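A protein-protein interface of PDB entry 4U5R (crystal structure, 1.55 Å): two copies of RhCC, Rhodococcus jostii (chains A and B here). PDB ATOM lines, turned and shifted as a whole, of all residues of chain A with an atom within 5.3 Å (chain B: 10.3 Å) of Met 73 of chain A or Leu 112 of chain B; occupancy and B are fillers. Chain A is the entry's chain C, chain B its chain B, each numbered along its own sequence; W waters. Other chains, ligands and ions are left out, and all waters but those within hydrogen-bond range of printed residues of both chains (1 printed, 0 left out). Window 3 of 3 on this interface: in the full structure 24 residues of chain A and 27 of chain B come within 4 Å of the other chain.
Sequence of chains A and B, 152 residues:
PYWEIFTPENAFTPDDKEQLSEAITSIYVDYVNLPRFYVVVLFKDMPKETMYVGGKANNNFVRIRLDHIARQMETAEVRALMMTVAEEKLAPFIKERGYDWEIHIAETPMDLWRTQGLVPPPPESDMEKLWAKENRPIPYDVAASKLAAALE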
ATOM      1  N   HIS A  68     -17.661  24.282 -31.304  1.00  0.00           N
ATOM      2  CA  HIS A  68     -16.494  23.764 -30.604  1.00  0.00           C
ATOM      3  C   HIS A  68     -15.508  23.261 -31.631  1.00  0.00           C
ATOM      4  O   HIS A  68     -15.856  22.399 -32.444  1.00  0.00           O
ATOM      5  CB  HIS A  68     -16.876  22.634 -29.655  1.00  0.00           C
ATOM      6  CG  HIS A  68     -17.248  23.091 -28.278  1.00  0.00           C
ATOM      7  ND1 HIS A  68     -17.460  22.203 -27.244  1.00  0.00           N
ATOM      8  CD2 HIS A  68     -17.422  24.328 -27.754  1.00  0.00           C
ATOM      9  CE1 HIS A  68     -17.753  22.872 -26.143  1.00  0.00           C
ATOM     10  NE2 HIS A  68     -17.753  24.162 -26.430  1.00  0.00           N
ATOM     11  N   ARG A  71     -11.636  21.038 -29.309  1.00  0.00           N
ATOM     12  CA  ARG A  71     -11.867  19.760 -28.635  1.00  0.00           C
ATOM     13  C   ARG A  71     -13.103  19.066 -29.185  1.00  0.00           C
ATOM     14  O   ARG A  71     -14.062  19.716 -29.608  1.00  0.00           O
ATOM     15  CB  ARG A  71     -12.047  19.944 -27.122  1.00  0.00           C
ATOM     16  CG  ARG A  71     -10.808  20.387 -26.356  1.00  0.00           C
ATOM     17  CD  ARG A  71      -9.718  19.317 -26.336  1.00  0.00           C
ATOM     18  NE  ARG A  71      -8.693  19.633 -25.344  1.00  0.00           N
ATOM     19  CZ  ARG A  71      -7.740  20.546 -25.519  1.00  0.00           C
ATOM     20  NH1 ARG A  71      -6.849  20.776 -24.560  1.00  0.00           N
ATOM     21  NH2 ARG A  71      -7.678  21.234 -26.656  1.00  0.00           N
ATOM     22  N   GLN A  72     -13.069  17.740 -29.156  1.00  0.00           N
ATOM     23  CA  GLN A  72     -14.239  16.931 -29.446  1.00  0.00           C
ATOM     24  C   GLN A  72     -14.673  16.273 -28.149  1.00  0.00           C
ATOM     25  O   GLN A  72     -13.839  15.781 -27.394  1.00  0.00           O
ATOM     26  CB  GLN A  72     -13.937  15.879 -30.516  1.00  0.00           C
ATOM     27  CG  GLN A  72     -13.957  16.413 -31.941  1.00  0.00           C
ATOM     28  CD  GLN A  72     -12.956  17.534 -32.168  1.00  0.00           C
ATOM     29  OE1 GLN A  72     -11.780  17.416 -31.815  1.00  0.00           O
ATOM     30  NE2 GLN A  72     -13.423  18.633 -32.751  1.00  0.00           N
ATOM     31  N   MET A  73     -15.970  16.280 -27.878  1.00  0.00           N
ATOM     32  CA  MET A  73     -16.478  15.646 -26.670  1.00  0.00           C
ATOM     33  C   MET A  73     -16.991  14.256 -27.015  1.00  0.00           C
ATOM     34  O   MET A  73     -17.990  14.110 -27.712  1.00  0.00           O
ATOM     35  CB  MET A  73     -17.567  16.504 -26.036  1.00  0.00           C
ATOM     36  CG  MET A  73     -17.050  17.814 -25.491  1.00  0.00           C
ATOM     37  SD  MET A  73     -18.375  18.876 -24.915  1.00  0.00           S
ATOM     38  CE  MET A  73     -19.268  19.160 -26.439  1.00  0.00           C
ATOM     39  N   GLU A  74     -16.307  13.231 -26.518  1.00  0.00           N
ATOM     40  CA  GLU A  74     -16.493  11.886 -27.058  1.00  0.00           C
ATOM     41  C   GLU A  74     -17.436  10.968 -26.273  1.00  0.00           C
ATOM     42  O   GLU A  74     -17.871   9.948 -26.807  1.00  0.00           O
ATOM     43  CB  GLU A  74     -15.126  11.209 -27.207  1.00  0.00           C
ATOM     44  CG  GLU A  74     -14.209  11.940 -28.185  1.00  0.00           C
ATOM     45  CD  GLU A  74     -12.903  11.215 -28.427  1.00  0.00           C
ATOM     46  OE1 GLU A  74     -12.875   9.974 -28.280  1.00  0.00           O
ATOM     47  OE2 GLU A  74     -11.905  11.885 -28.770  1.00  0.00           O
ATOM     48  N   THR A  75     -17.757  11.319 -25.028  1.00  0.00           N
ATOM     49  CA  THR A  75     -18.655  10.500 -24.207  1.00  0.00           C
ATOM     50  C   THR A  75     -19.912  11.263 -23.790  1.00  0.00           C
ATOM     51  O   THR A  75     -19.896  12.492 -23.679  1.00  0.00           O
ATOM     52  CB  THR A  75     -17.959   9.991 -22.932  1.00  0.00           C
ATOM     53  OG1 THR A  75     -17.736  11.087 -22.028  1.00  0.00           O
ATOM     54  CG2 THR A  75     -16.631   9.319 -23.273  1.00  0.00           C
ATOM     55  N   VAL A  78     -19.308  13.495 -20.631  1.00  0.00           N
ATOM     56  CA  VAL A  78     -18.607  14.764 -20.839  1.00  0.00           C
ATOM     57  C   VAL A  78     -19.511  15.773 -21.541  1.00  0.00           C
ATOM     58  O   VAL A  78     -19.520  16.959 -21.209  1.00  0.00           O
ATOM     59  CB  VAL A  78     -17.310  14.568 -21.658  1.00  0.00           C
ATOM     60  CG1 VAL A  78     -16.771  15.902 -22.163  1.00  0.00           C
ATOM     61  CG2 VAL A  78     -16.263  13.845 -20.816  1.00  0.00           C
ATOM     62  N   ARG A  79     -20.281  15.294 -22.510  1.00  0.00           N
ATOM     63  CA  ARG A  79     -21.188  16.155 -23.251  1.00  0.00           C
ATOM     64  C   ARG A  79     -22.296  16.696 -22.348  1.00  0.00           C
ATOM     65  O   ARG A  79     -22.664  17.874 -22.430  1.00  0.00           O
ATOM     66  CB  ARG A  79     -21.753  15.389 -24.442  1.00  0.00           C
ATOM     67  CG  ARG A  79     -20.638  15.052 -25.427  1.00  0.00           C
ATOM     68  CD  ARG A  79     -20.981  13.903 -26.345  1.00  0.00           C
ATOM     69  NE  ARG A  79     -21.939  14.307 -27.365  1.00  0.00           N
ATOM     70  CZ  ARG A  79     -21.612  14.899 -28.507  1.00  0.00           C
ATOM     71  NH1 ARG A  79     -20.342  15.168 -28.785  1.00  0.00           N
ATOM     72  NH2 ARG A  79     -22.566  15.235 -29.365  1.00  0.00           N
ATOM     73  N   MET A  82     -20.670  19.367 -20.117  1.00  0.00           N
ATOM     74  CA  MET A  82     -20.529  20.630 -20.832  1.00  0.00           C
ATOM     75  C   MET A  82     -21.821  21.444 -20.766  1.00  0.00           C
ATOM     76  O   MET A  82     -21.790  22.624 -20.420  1.00  0.00           O
ATOM     77  CB  MET A  82     -20.129  20.391 -22.292  1.00  0.00           C
ATOM     78  CG  MET A  82     -20.135  21.649 -23.157  1.00  0.00           C
ATOM     79  SD  MET A  82     -18.867  22.790 -22.620  1.00  0.00           S
ATOM     80  CE  MET A  82     -19.641  24.359 -23.032  1.00  0.00           C
ATOM     81  N   MET A  83     -22.957  20.821 -21.073  1.00  0.00           N
ATOM     82  CA  MET A  83     -24.229  21.550 -21.031  1.00  0.00           C
ATOM     83  C   MET A  83     -24.577  22.019 -19.621  1.00  0.00           C
ATOM     84  O   MET A  83     -25.053  23.153 -19.421  1.00  0.00           O
ATOM     85  CB  MET A  83     -25.373  20.690 -21.590  1.00  0.00           C
ATOM     86  CG  MET A  83     -25.124  20.167 -23.008  1.00  0.00           C
ATOM     87  SD  MET A  83     -24.575  21.399 -24.214  1.00  0.00           S
ATOM     88  CE  MET A  83     -26.012  22.462 -24.295  1.00  0.00           C
ATOM     89  N   ILE A 103     -30.022  27.151 -25.991  1.00  0.00           N
ATOM     90  CA  ILE A 103     -28.613  27.008 -26.351  1.00  0.00           C
ATOM     91  C   ILE A 103     -28.366  25.706 -27.095  1.00  0.00           C
ATOM     92  O   ILE A 103     -28.967  24.683 -26.773  1.00  0.00           O
ATOM     93  CB  ILE A 103     -27.709  27.049 -25.097  1.00  0.00           C
ATOM     94  CG1 ILE A 103     -26.234  26.973 -25.501  1.00  0.00           C
ATOM     95  CG2 ILE A 103     -28.050  25.890 -24.134  1.00  0.00           C
ATOM     96  CD1 ILE A 103     -25.278  27.203 -24.316  1.00  0.00           C
ATOM     97  N   HIS A 104     -27.516  25.746 -28.115  1.00  0.00           N
ATOM     98  CA  HIS A 104     -27.006  24.510 -28.715  1.00  0.00           C
ATOM     99  C   HIS A 104     -25.577  24.651 -29.208  1.00  0.00           C
ATOM    100  O   HIS A 104     -25.074  25.761 -29.423  1.00  0.00           O
ATOM    101  CB  HIS A 104     -27.923  24.000 -29.848  1.00  0.00           C
ATOM    102  CG  HIS A 104     -27.846  24.759 -31.143  1.00  0.00           C
ATOM    103  ND1 HIS A 104     -28.371  26.025 -31.296  1.00  0.00           N
ATOM    104  CD2 HIS A 104     -27.423  24.377 -32.374  1.00  0.00           C
ATOM    105  CE1 HIS A 104     -28.235  26.408 -32.553  1.00  0.00           C
ATOM    106  NE2 HIS A 104     -27.659  25.427 -33.229  1.00  0.00           N
ATOM    107  N   ILE A 105     -24.925  23.493 -29.342  1.00  0.00           N
ATOM    108  CA  ILE A 105     -23.532  23.371 -29.766  1.00  0.00           C
ATOM    109  C   ILE A 105     -23.397  22.568 -31.048  1.00  0.00           C
ATOM    110  O   ILE A 105     -24.076  21.552 -31.229  1.00  0.00           O
ATOM    111  CB  ILE A 105     -22.682  22.685 -28.689  1.00  0.00           C
ATOM    112  CG1 ILE A 105     -23.002  23.274 -27.320  1.00  0.00           C
ATOM    113  CG2 ILE A 105     -21.189  22.697 -29.041  1.00  0.00           C
ATOM    114  CD1 ILE A 105     -22.089  22.762 -26.246  1.00  0.00           C
ATOM    115  N   GLU A 107     -20.073  20.900 -33.430  1.00  0.00           N
ATOM    116  CA  GLU A 107     -18.646  20.602 -33.483  1.00  0.00           C
ATOM    117  C   GLU A 107     -18.159  20.704 -34.923  1.00  0.00           C
ATOM    118  O   GLU A 107     -18.777  20.171 -35.856  1.00  0.00           O
ATOM    119  CB  GLU A 107     -18.355  19.218 -32.874  1.00  0.00           C
ATOM    120  CG  GLU A 107     -18.573  19.202 -31.350  1.00  0.00           C
ATOM    121  CD  GLU A 107     -18.429  17.823 -30.707  1.00  0.00           C
ATOM    122  OE1 GLU A 107     -18.986  16.841 -31.244  1.00  0.00           O
ATOM    123  OE2 GLU A 107     -17.762  17.725 -29.656  1.00  0.00           O
ATOM    124  N   ASP B  67     -29.964  25.350 -38.620  1.00  0.00           N
ATOM    125  CA  ASP B  67     -29.597  24.085 -37.975  1.00  0.00           C
ATOM    126  C   ASP B  67     -30.820  23.259 -37.627  1.00  0.00           C
ATOM    127  O   ASP B  67     -31.823  23.791 -37.137  1.00  0.00           O
ATOM    128  CB  ASP B  67     -28.816  24.312 -36.670  1.00  0.00           C
ATOM    129  CG  ASP B  67     -27.438  24.931 -36.880  1.00  0.00           C
ATOM    130  OD1 ASP B  67     -26.783  24.694 -37.908  1.00  0.00           O
ATOM    131  OD2 ASP B  67     -26.980  25.635 -35.963  1.00  0.00           O
ATOM    132  N   HIS B  68     -30.722  21.952 -37.842  1.00  0.00           N
ATOM    133  CA  HIS B  68     -31.691  21.011 -37.308  1.00  0.00           C
ATOM    134  C   HIS B  68     -31.041  20.298 -36.146  1.00  0.00           C
ATOM    135  O   HIS B  68     -29.945  19.750 -36.299  1.00  0.00           O
ATOM    136  CB  HIS B  68     -32.125  20.008 -38.368  1.00  0.00           C
ATOM    137  CG  HIS B  68     -33.206  20.508 -39.271  1.00  0.00           C
ATOM    138  ND1 HIS B  68     -33.779  19.714 -40.236  1.00  0.00           N
ATOM    139  CD2 HIS B  68     -33.841  21.706 -39.343  1.00  0.00           C
ATOM    140  CE1 HIS B  68     -34.719  20.394 -40.868  1.00  0.00           C
ATOM    141  NE2 HIS B  68     -34.776  21.608 -40.346  1.00  0.00           N
ATOM    142  N   ILE B  69     -31.720  20.314 -35.002  1.00  0.00           N
ATOM    143  CA  ILE B  69     -31.184  19.794 -33.752  1.00  0.00           C
ATOM    144  C   ILE B  69     -31.987  18.627 -33.215  1.00  0.00           C
ATOM    145  O   ILE B  69     -31.419  17.644 -32.749  1.00  0.00           O
ATOM    146  CB  ILE B  69     -31.152  20.890 -32.677  1.00  0.00           C
ATOM    147  CG1 ILE B  69     -30.562  22.175 -33.266  1.00  0.00           C
ATOM    148  CG2 ILE B  69     -30.366  20.414 -31.459  1.00  0.00           C
ATOM    149  CD1 ILE B  69     -31.002  23.462 -32.535  1.00  0.00           C
ATOM    150  N   ALA B  70     -33.310  18.739 -33.280  1.00  0.00           N
ATOM    151  CA  ALA B  70     -34.186  17.776 -32.620  1.00  0.00           C
ATOM    152  C   ALA B  70     -34.265  16.463 -33.396  1.00  0.00           C
ATOM    153  O   ALA B  70     -34.265  15.383 -32.805  1.00  0.00           O
ATOM    154  CB  ALA B  70     -35.579  18.376 -32.428  1.00  0.00           C
ATOM    155  N   GLU B 107     -27.007  19.745 -39.691  1.00  0.00           N
ATOM    156  CA  GLU B 107     -27.546  18.946 -38.605  1.00  0.00           C
ATOM    157  C   GLU B 107     -26.505  18.956 -37.491  1.00  0.00           C
ATOM    158  O   GLU B 107     -25.321  18.705 -37.741  1.00  0.00           O
ATOM    159  CB  GLU B 107     -27.875  17.518 -39.070  1.00  0.00           C
ATOM    160  CG  GLU B 107     -28.899  17.475 -40.205  1.00  0.00           C
ATOM    161  CD  GLU B 107     -29.320  16.061 -40.594  1.00  0.00           C
ATOM    162  OE1 GLU B 107     -28.438  15.229 -40.891  1.00  0.00           O
ATOM    163  OE2 GLU B 107     -30.535  15.784 -40.605  1.00  0.00           O
ATOM    164  N   THR B 108     -26.949  19.293 -36.282  1.00  0.00           N
ATOM    165  CA  THR B 108     -26.072  19.418 -35.119  1.00  0.00           C
ATOM    166  C   THR B 108     -26.539  18.431 -34.043  1.00  0.00           C
ATOM    167  O   THR B 108     -27.679  17.953 -34.089  1.00  0.00           O
ATOM    168  CB  THR B 108     -26.048  20.877 -34.566  1.00  0.00           C
ATOM    169  OG1 THR B 108     -27.306  21.186 -33.963  1.00  0.00           O
ATOM    170  CG2 THR B 108     -25.779  21.896 -35.690  1.00  0.00           C
ATOM    171  N   PRO B 109     -25.645  18.069 -33.101  1.00  0.00           N
ATOM    172  CA  PRO B 109     -25.946  16.987 -32.144  1.00  0.00           C
ATOM    173  C   PRO B 109     -27.122  17.252 -31.204  1.00  0.00           C
ATOM    174  O   PRO B 109     -27.131  18.239 -30.454  1.00  0.00           O
ATOM    175  CB  PRO B 109     -24.654  16.868 -31.329  1.00  0.00           C
ATOM    176  CG  PRO B 109     -23.600  17.419 -32.189  1.00  0.00           C
ATOM    177  CD  PRO B 109     -24.231  18.483 -33.039  1.00  0.00           C
ATOM    178  N   MET B 110     -28.095  16.345 -31.218  1.00  0.00           N
ATOM    179  CA  MET B 110     -29.296  16.498 -30.399  1.00  0.00           C
ATOM    180  C   MET B 110     -29.007  16.602 -28.901  1.00  0.00           C
ATOM    181  O   MET B 110     -29.768  17.228 -28.165  1.00  0.00           O
ATOM    182  CB  MET B 110     -30.252  15.329 -30.660  1.00  0.00           C
ATOM    183  CG  MET B 110     -31.639  15.502 -30.064  1.00  0.00           C
ATOM    184  SD  MET B 110     -32.707  14.116 -30.510  1.00  0.00           S
ATOM    185  CE  MET B 110     -31.795  12.743 -29.810  1.00  0.00           C
ATOM    186  N   ASP B 111     -27.917  15.988 -28.448  1.00  0.00           N
ATOM    187  CA  ASP B 111     -27.623  15.941 -27.019  1.00  0.00           C
ATOM    188  C   ASP B 111     -26.829  17.153 -26.540  1.00  0.00           C
ATOM    189  O   ASP B 111     -26.496  17.253 -25.362  1.00  0.00           O
ATOM    190  CB  ASP B 111     -26.873  14.644 -26.673  1.00  0.00           C
ATOM    191  CG  ASP B 111     -25.526  14.516 -27.383  1.00  0.00           C
ATOM    192  OD1 ASP B 111     -25.230  15.282 -28.326  1.00  0.00           O
ATOM    193  OD2 ASP B 111     -24.752  13.612 -26.998  1.00  0.00           O
ATOM    194  N   LEU B 112     -26.542  18.085 -27.441  1.00  0.00           N
ATOM    195  CA  LEU B 112     -25.805  19.294 -27.055  1.00  0.00           C
ATOM    196  C   LEU B 112     -26.718  20.506 -27.159  1.00  0.00           C
ATOM    197  O   LEU B 112     -26.375  21.508 -27.767  1.00  0.00           O
ATOM    198  CB  LEU B 112     -24.551  19.483 -27.917  1.00  0.00           C
ATOM    199  CG  LEU B 112     -23.466  18.417 -27.757  1.00  0.00           C
ATOM    200  CD1 LEU B 112     -22.268  18.743 -28.633  1.00  0.00           C
ATOM    201  CD2 LEU B 112     -23.049  18.337 -26.297  1.00  0.00           C
ATOM    202  N   TRP B 113     -27.871  20.405 -26.511  1.00  0.00           N
ATOM    203  CA  TRP B 113     -28.979  21.309 -26.749  1.00  0.00           C
ATOM    204  C   TRP B 113     -29.834  21.384 -25.497  1.00  0.00           C
ATOM    205  O   TRP B 113     -30.228  20.363 -24.960  1.00  0.00           O
ATOM    206  CB  TRP B 113     -29.783  20.811 -27.956  1.00  0.00           C
ATOM    207  CG  TRP B 113     -31.122  21.457 -28.155  1.00  0.00           C
ATOM    208  CD1 TRP B 113     -31.429  22.791 -28.054  1.00  0.00           C
ATOM    209  CD2 TRP B 113     -32.346  20.793 -28.495  1.00  0.00           C
ATOM    210  NE1 TRP B 113     -32.761  22.990 -28.326  1.00  0.00           N
ATOM    211  CE2 TRP B 113     -33.345  21.779 -28.596  1.00  0.00           C
ATOM    212  CE3 TRP B 113     -32.687  19.456 -28.729  1.00  0.00           C
ATOM    213  CZ2 TRP B 113     -34.671  21.472 -28.907  1.00  0.00           C
ATOM    214  CZ3 TRP B 113     -34.001  19.153 -29.037  1.00  0.00           C
ATOM    215  CH2 TRP B 113     -34.977  20.157 -29.129  1.00  0.00           C
ATOM    216  N   ARG B 114     -30.105  22.591 -25.014  1.00  0.00           N
ATOM    217  CA  ARG B 114     -30.997  22.757 -23.881  1.00  0.00           C
ATOM    218  C   ARG B 114     -31.949  23.888 -24.213  1.00  0.00           C
ATOM    219  O   ARG B 114     -31.571  24.847 -24.892  1.00  0.00           O
ATOM    220  CB  ARG B 114     -30.223  23.073 -22.588  1.00  0.00           C
ATOM    221  CG  ARG B 114     -29.171  22.037 -22.185  1.00  0.00           C
ATOM    222  CD  ARG B 114     -29.854  20.781 -21.653  1.00  0.00           C
ATOM    223  NE  ARG B 114     -28.912  19.802 -21.121  1.00  0.00           N
ATOM    224  CZ  ARG B 114     -28.407  18.782 -21.812  1.00  0.00           C
ATOM    225  NH1 ARG B 114     -28.727  18.595 -23.096  1.00  0.00           N
ATOM    226  NH2 ARG B 114     -27.561  17.946 -21.217  1.00  0.00           N
ATOM    227  N   THR B 115     -33.179  23.800 -23.736  1.00  0.00           N
ATOM    228  CA  THR B 115     -34.082  24.933 -23.854  1.00  0.00           C
ATOM    229  C   THR B 115     -34.650  25.261 -22.470  1.00  0.00           C
ATOM    230  O   THR B 115     -35.089  24.372 -21.748  1.00  0.00           O
ATOM    231  CB  THR B 115     -35.195  24.676 -24.887  1.00  0.00           C
ATOM    232  OG1 THR B 115     -35.947  25.891 -25.084  1.00  0.00           O
ATOM    233  CG2 THR B 115     -36.102  23.510 -24.461  1.00  0.00           C
ATOM    234  N   LEU B 118     -33.422  23.111 -19.790  1.00  0.00           N
ATOM    235  CA  LEU B 118     -33.940  21.745 -19.675  1.00  0.00           C
ATOM    236  C   LEU B 118     -33.471  20.854 -20.816  1.00  0.00           C
ATOM    237  O   LEU B 118     -33.295  21.319 -21.941  1.00  0.00           O
ATOM    238  CB  LEU B 118     -35.476  21.749 -19.643  1.00  0.00           C
ATOM    239  CG  LEU B 118     -36.174  22.550 -18.540  1.00  0.00           C
ATOM    240  CD1 LEU B 118     -37.684  22.581 -18.749  1.00  0.00           C
ATOM    241  CD2 LEU B 118     -35.819  21.964 -17.172  1.00  0.00           C
ATOM    242  N   VAL B 119     -33.306  19.569 -20.518  1.00  0.00           N
ATOM    243  CA  VAL B 119     -33.083  18.558 -21.545  1.00  0.00           C
ATOM    244  C   VAL B 119     -34.386  18.341 -22.299  1.00  0.00           C
ATOM    245  O   VAL B 119     -35.379  17.936 -21.700  1.00  0.00           O
ATOM    246  CB  VAL B 119     -32.617  17.218 -20.930  1.00  0.00           C
ATOM    247  CG1 VAL B 119     -32.516  16.122 -21.999  1.00  0.00           C
ATOM    248  CG2 VAL B 119     -31.301  17.391 -20.183  1.00  0.00           C
ATOM    249  N   PRO B 120     -34.399  18.621 -23.610  1.00  0.00           N
ATOM    250  CA  PRO B 120     -35.621  18.304 -24.353  1.00  0.00           C
ATOM    251  C   PRO B 120     -35.936  16.806 -24.322  1.00  0.00           C
ATOM    252  O   PRO B 120     -35.025  15.984 -24.293  1.00  0.00           O
ATOM    253  CB  PRO B 120     -35.297  18.789 -25.773  1.00  0.00           C
ATOM    254  CG  PRO B 120     -34.276  19.879 -25.550  1.00  0.00           C
ATOM    255  CD  PRO B 120     -33.423  19.348 -24.446  1.00  0.00           C
HETATM  256  O   HOH W   1     -26.743  20.920 -31.257  1.00  0.00           O
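N of Met 73 of chain A lies within hydrogen-bond range of OE2 of Glu 107 of chain A, 2.9 Å away.
The backbone carbonyl oxygen (O) of Asp 111 of chain B is in hydrogen-bond range of the guanidinium group (NH1) of Arg 114 of chain B, at 3.5 Å.
The guanidinium group (NH1) of Arg 79 of chain A lies within hydrogen-bond range of the backbone carbonyl oxygen (O) of Met 73 of chain A (2.8 Å).
The guanidinium group (NH1) of Arg 79 of chain A lies within salt-bridge range of the side-chain carboxylate (OE1) of Glu 107 of chain A, 3.3 Å away.
N of Thr 108 of chain B sits at hydrogen-bond distance from O of His 68 of chain B, 3.0 Å away.
Among the printed residues, merely in contact across the chains: His 104 of chain A with Leu 112 of chain B, Arg 79 of chain A with Pro 109 of chain B, Ile 103 of chain A with Trp 113 of chain B, Met 83 of chain A with Arg 114 of chain B, Met 83 of chain A with Leu 112 of chain B, Met 83 of chain A with Trp 113 of chain B, Ile 105 of chain A with Pro 109 of chain B, His 104 of chain A with Thr 108 of chain B, Arg 79 of chain A with Leu 112 of chain B, His 104 of chain A with Ile 69 of chain B, Met 73 of chain A with Leu 112 of chain B, Ile 105 of chain A with Thr 108 of chain B and Met 83 of chain A with Asp 111 of chain B.
Positions printed for both chains: 68 and 107.
Of the 17 pairs that touch across the chains among the printed residues, none has its exchanged pair printed and touching as well.
His 68 of chain A touches none of the printed residues of chain B.
No residue of chain B comes within 4 Å of Gln 72 of chain A.
Of the printed residues of chain B, Met 73 of chain A touches Leu 112 (3.7 Å).
No residue of chain B comes within 4 Å of Glu 74 of chain A.
No residue of chain B comes within 4 Å of Thr 75 of chain A.
Arg 79 of chain A touches just these residues of chain B: Pro 109 (3.3 Å), Asp 111 (2.9 Å) and Leu 112 (3.6 Å).
Printed residues of chain B within 4 Å of Ile 103 of chain A: Trp 113 (3.4 Å) and Arg 114 (3.0 Å).
Of the printed residues of chain B, His 104 of chain A touches Asp 67, Ile 69, Thr 108 and Leu 112.
Of the printed residues of chain A, Ile 69 of chain B touches His 104.
Of the printed residues of chain A, Thr 108 of chain B touches His 104 (3.6 Å) and Ile 105 (3.9 Å).
Leu 112 of chain B touches just these residues of chain A: Met 73, Arg 79, Met 83, His 104 and Ile 105.
Leu 118 of chain B touches none of the printed residues of chain A.
The nearest residue of chain B that does not touch Met 73 of chain A is Asp 111 of chain B (6.8 Å).
The nearest residue of chain A that does not touch Leu 112 of chain B is Ile 103 of chain A (4.2 Å).
The side-chain carboxylate of Asp 67 of chain B is in hydrogen-bond range of a ring nitrogen (NE2) of His 104 of chain A (2.8 Å).
The side-chain carboxylate (OD1) of Asp 111 of chain B lies within salt-bridge range of the guanidinium group (NH2) of Arg 79 of chain A (2.9 Å).
The backbone carbonyl oxygen of Leu 112 of chain B sits at hydrogen-bond distance from the backbone NH of Ile 105 of chain A (2.9 Å).
N of Arg 114 of chain B lies within hydrogen-bond range of O of Ile 103 of chain A, at 3.0 Å.
Printed residues of chain A that touch a printed residue of chain B: Met 73, Arg 79, Met 83, Ile 103, His 104 and Ile 105.
Hydrophobic or aromatic side chains of chain A that line the printed part of chain B: Met 73, Met 83, Ile 103, His 104 and Ile 105.
Among the printed residues, Asp or Glu carboxylates within 4 Å of a Lys or Arg side-chain nitrogen of the other chain: Arg 79 of chain A with Asp 111 of chain B (2.9 Å).
Water W1 lies within hydrogen-bond range of the backbone carbonyl oxygen (O) of Ile 105 of chain A (2.7 Å), the side-chain hydroxyl (OG1) of Thr 108 of chain B (2.8 Å) and the backbone carbonyl oxygen (O) of Pro 109 of chain B (2.8 Å).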
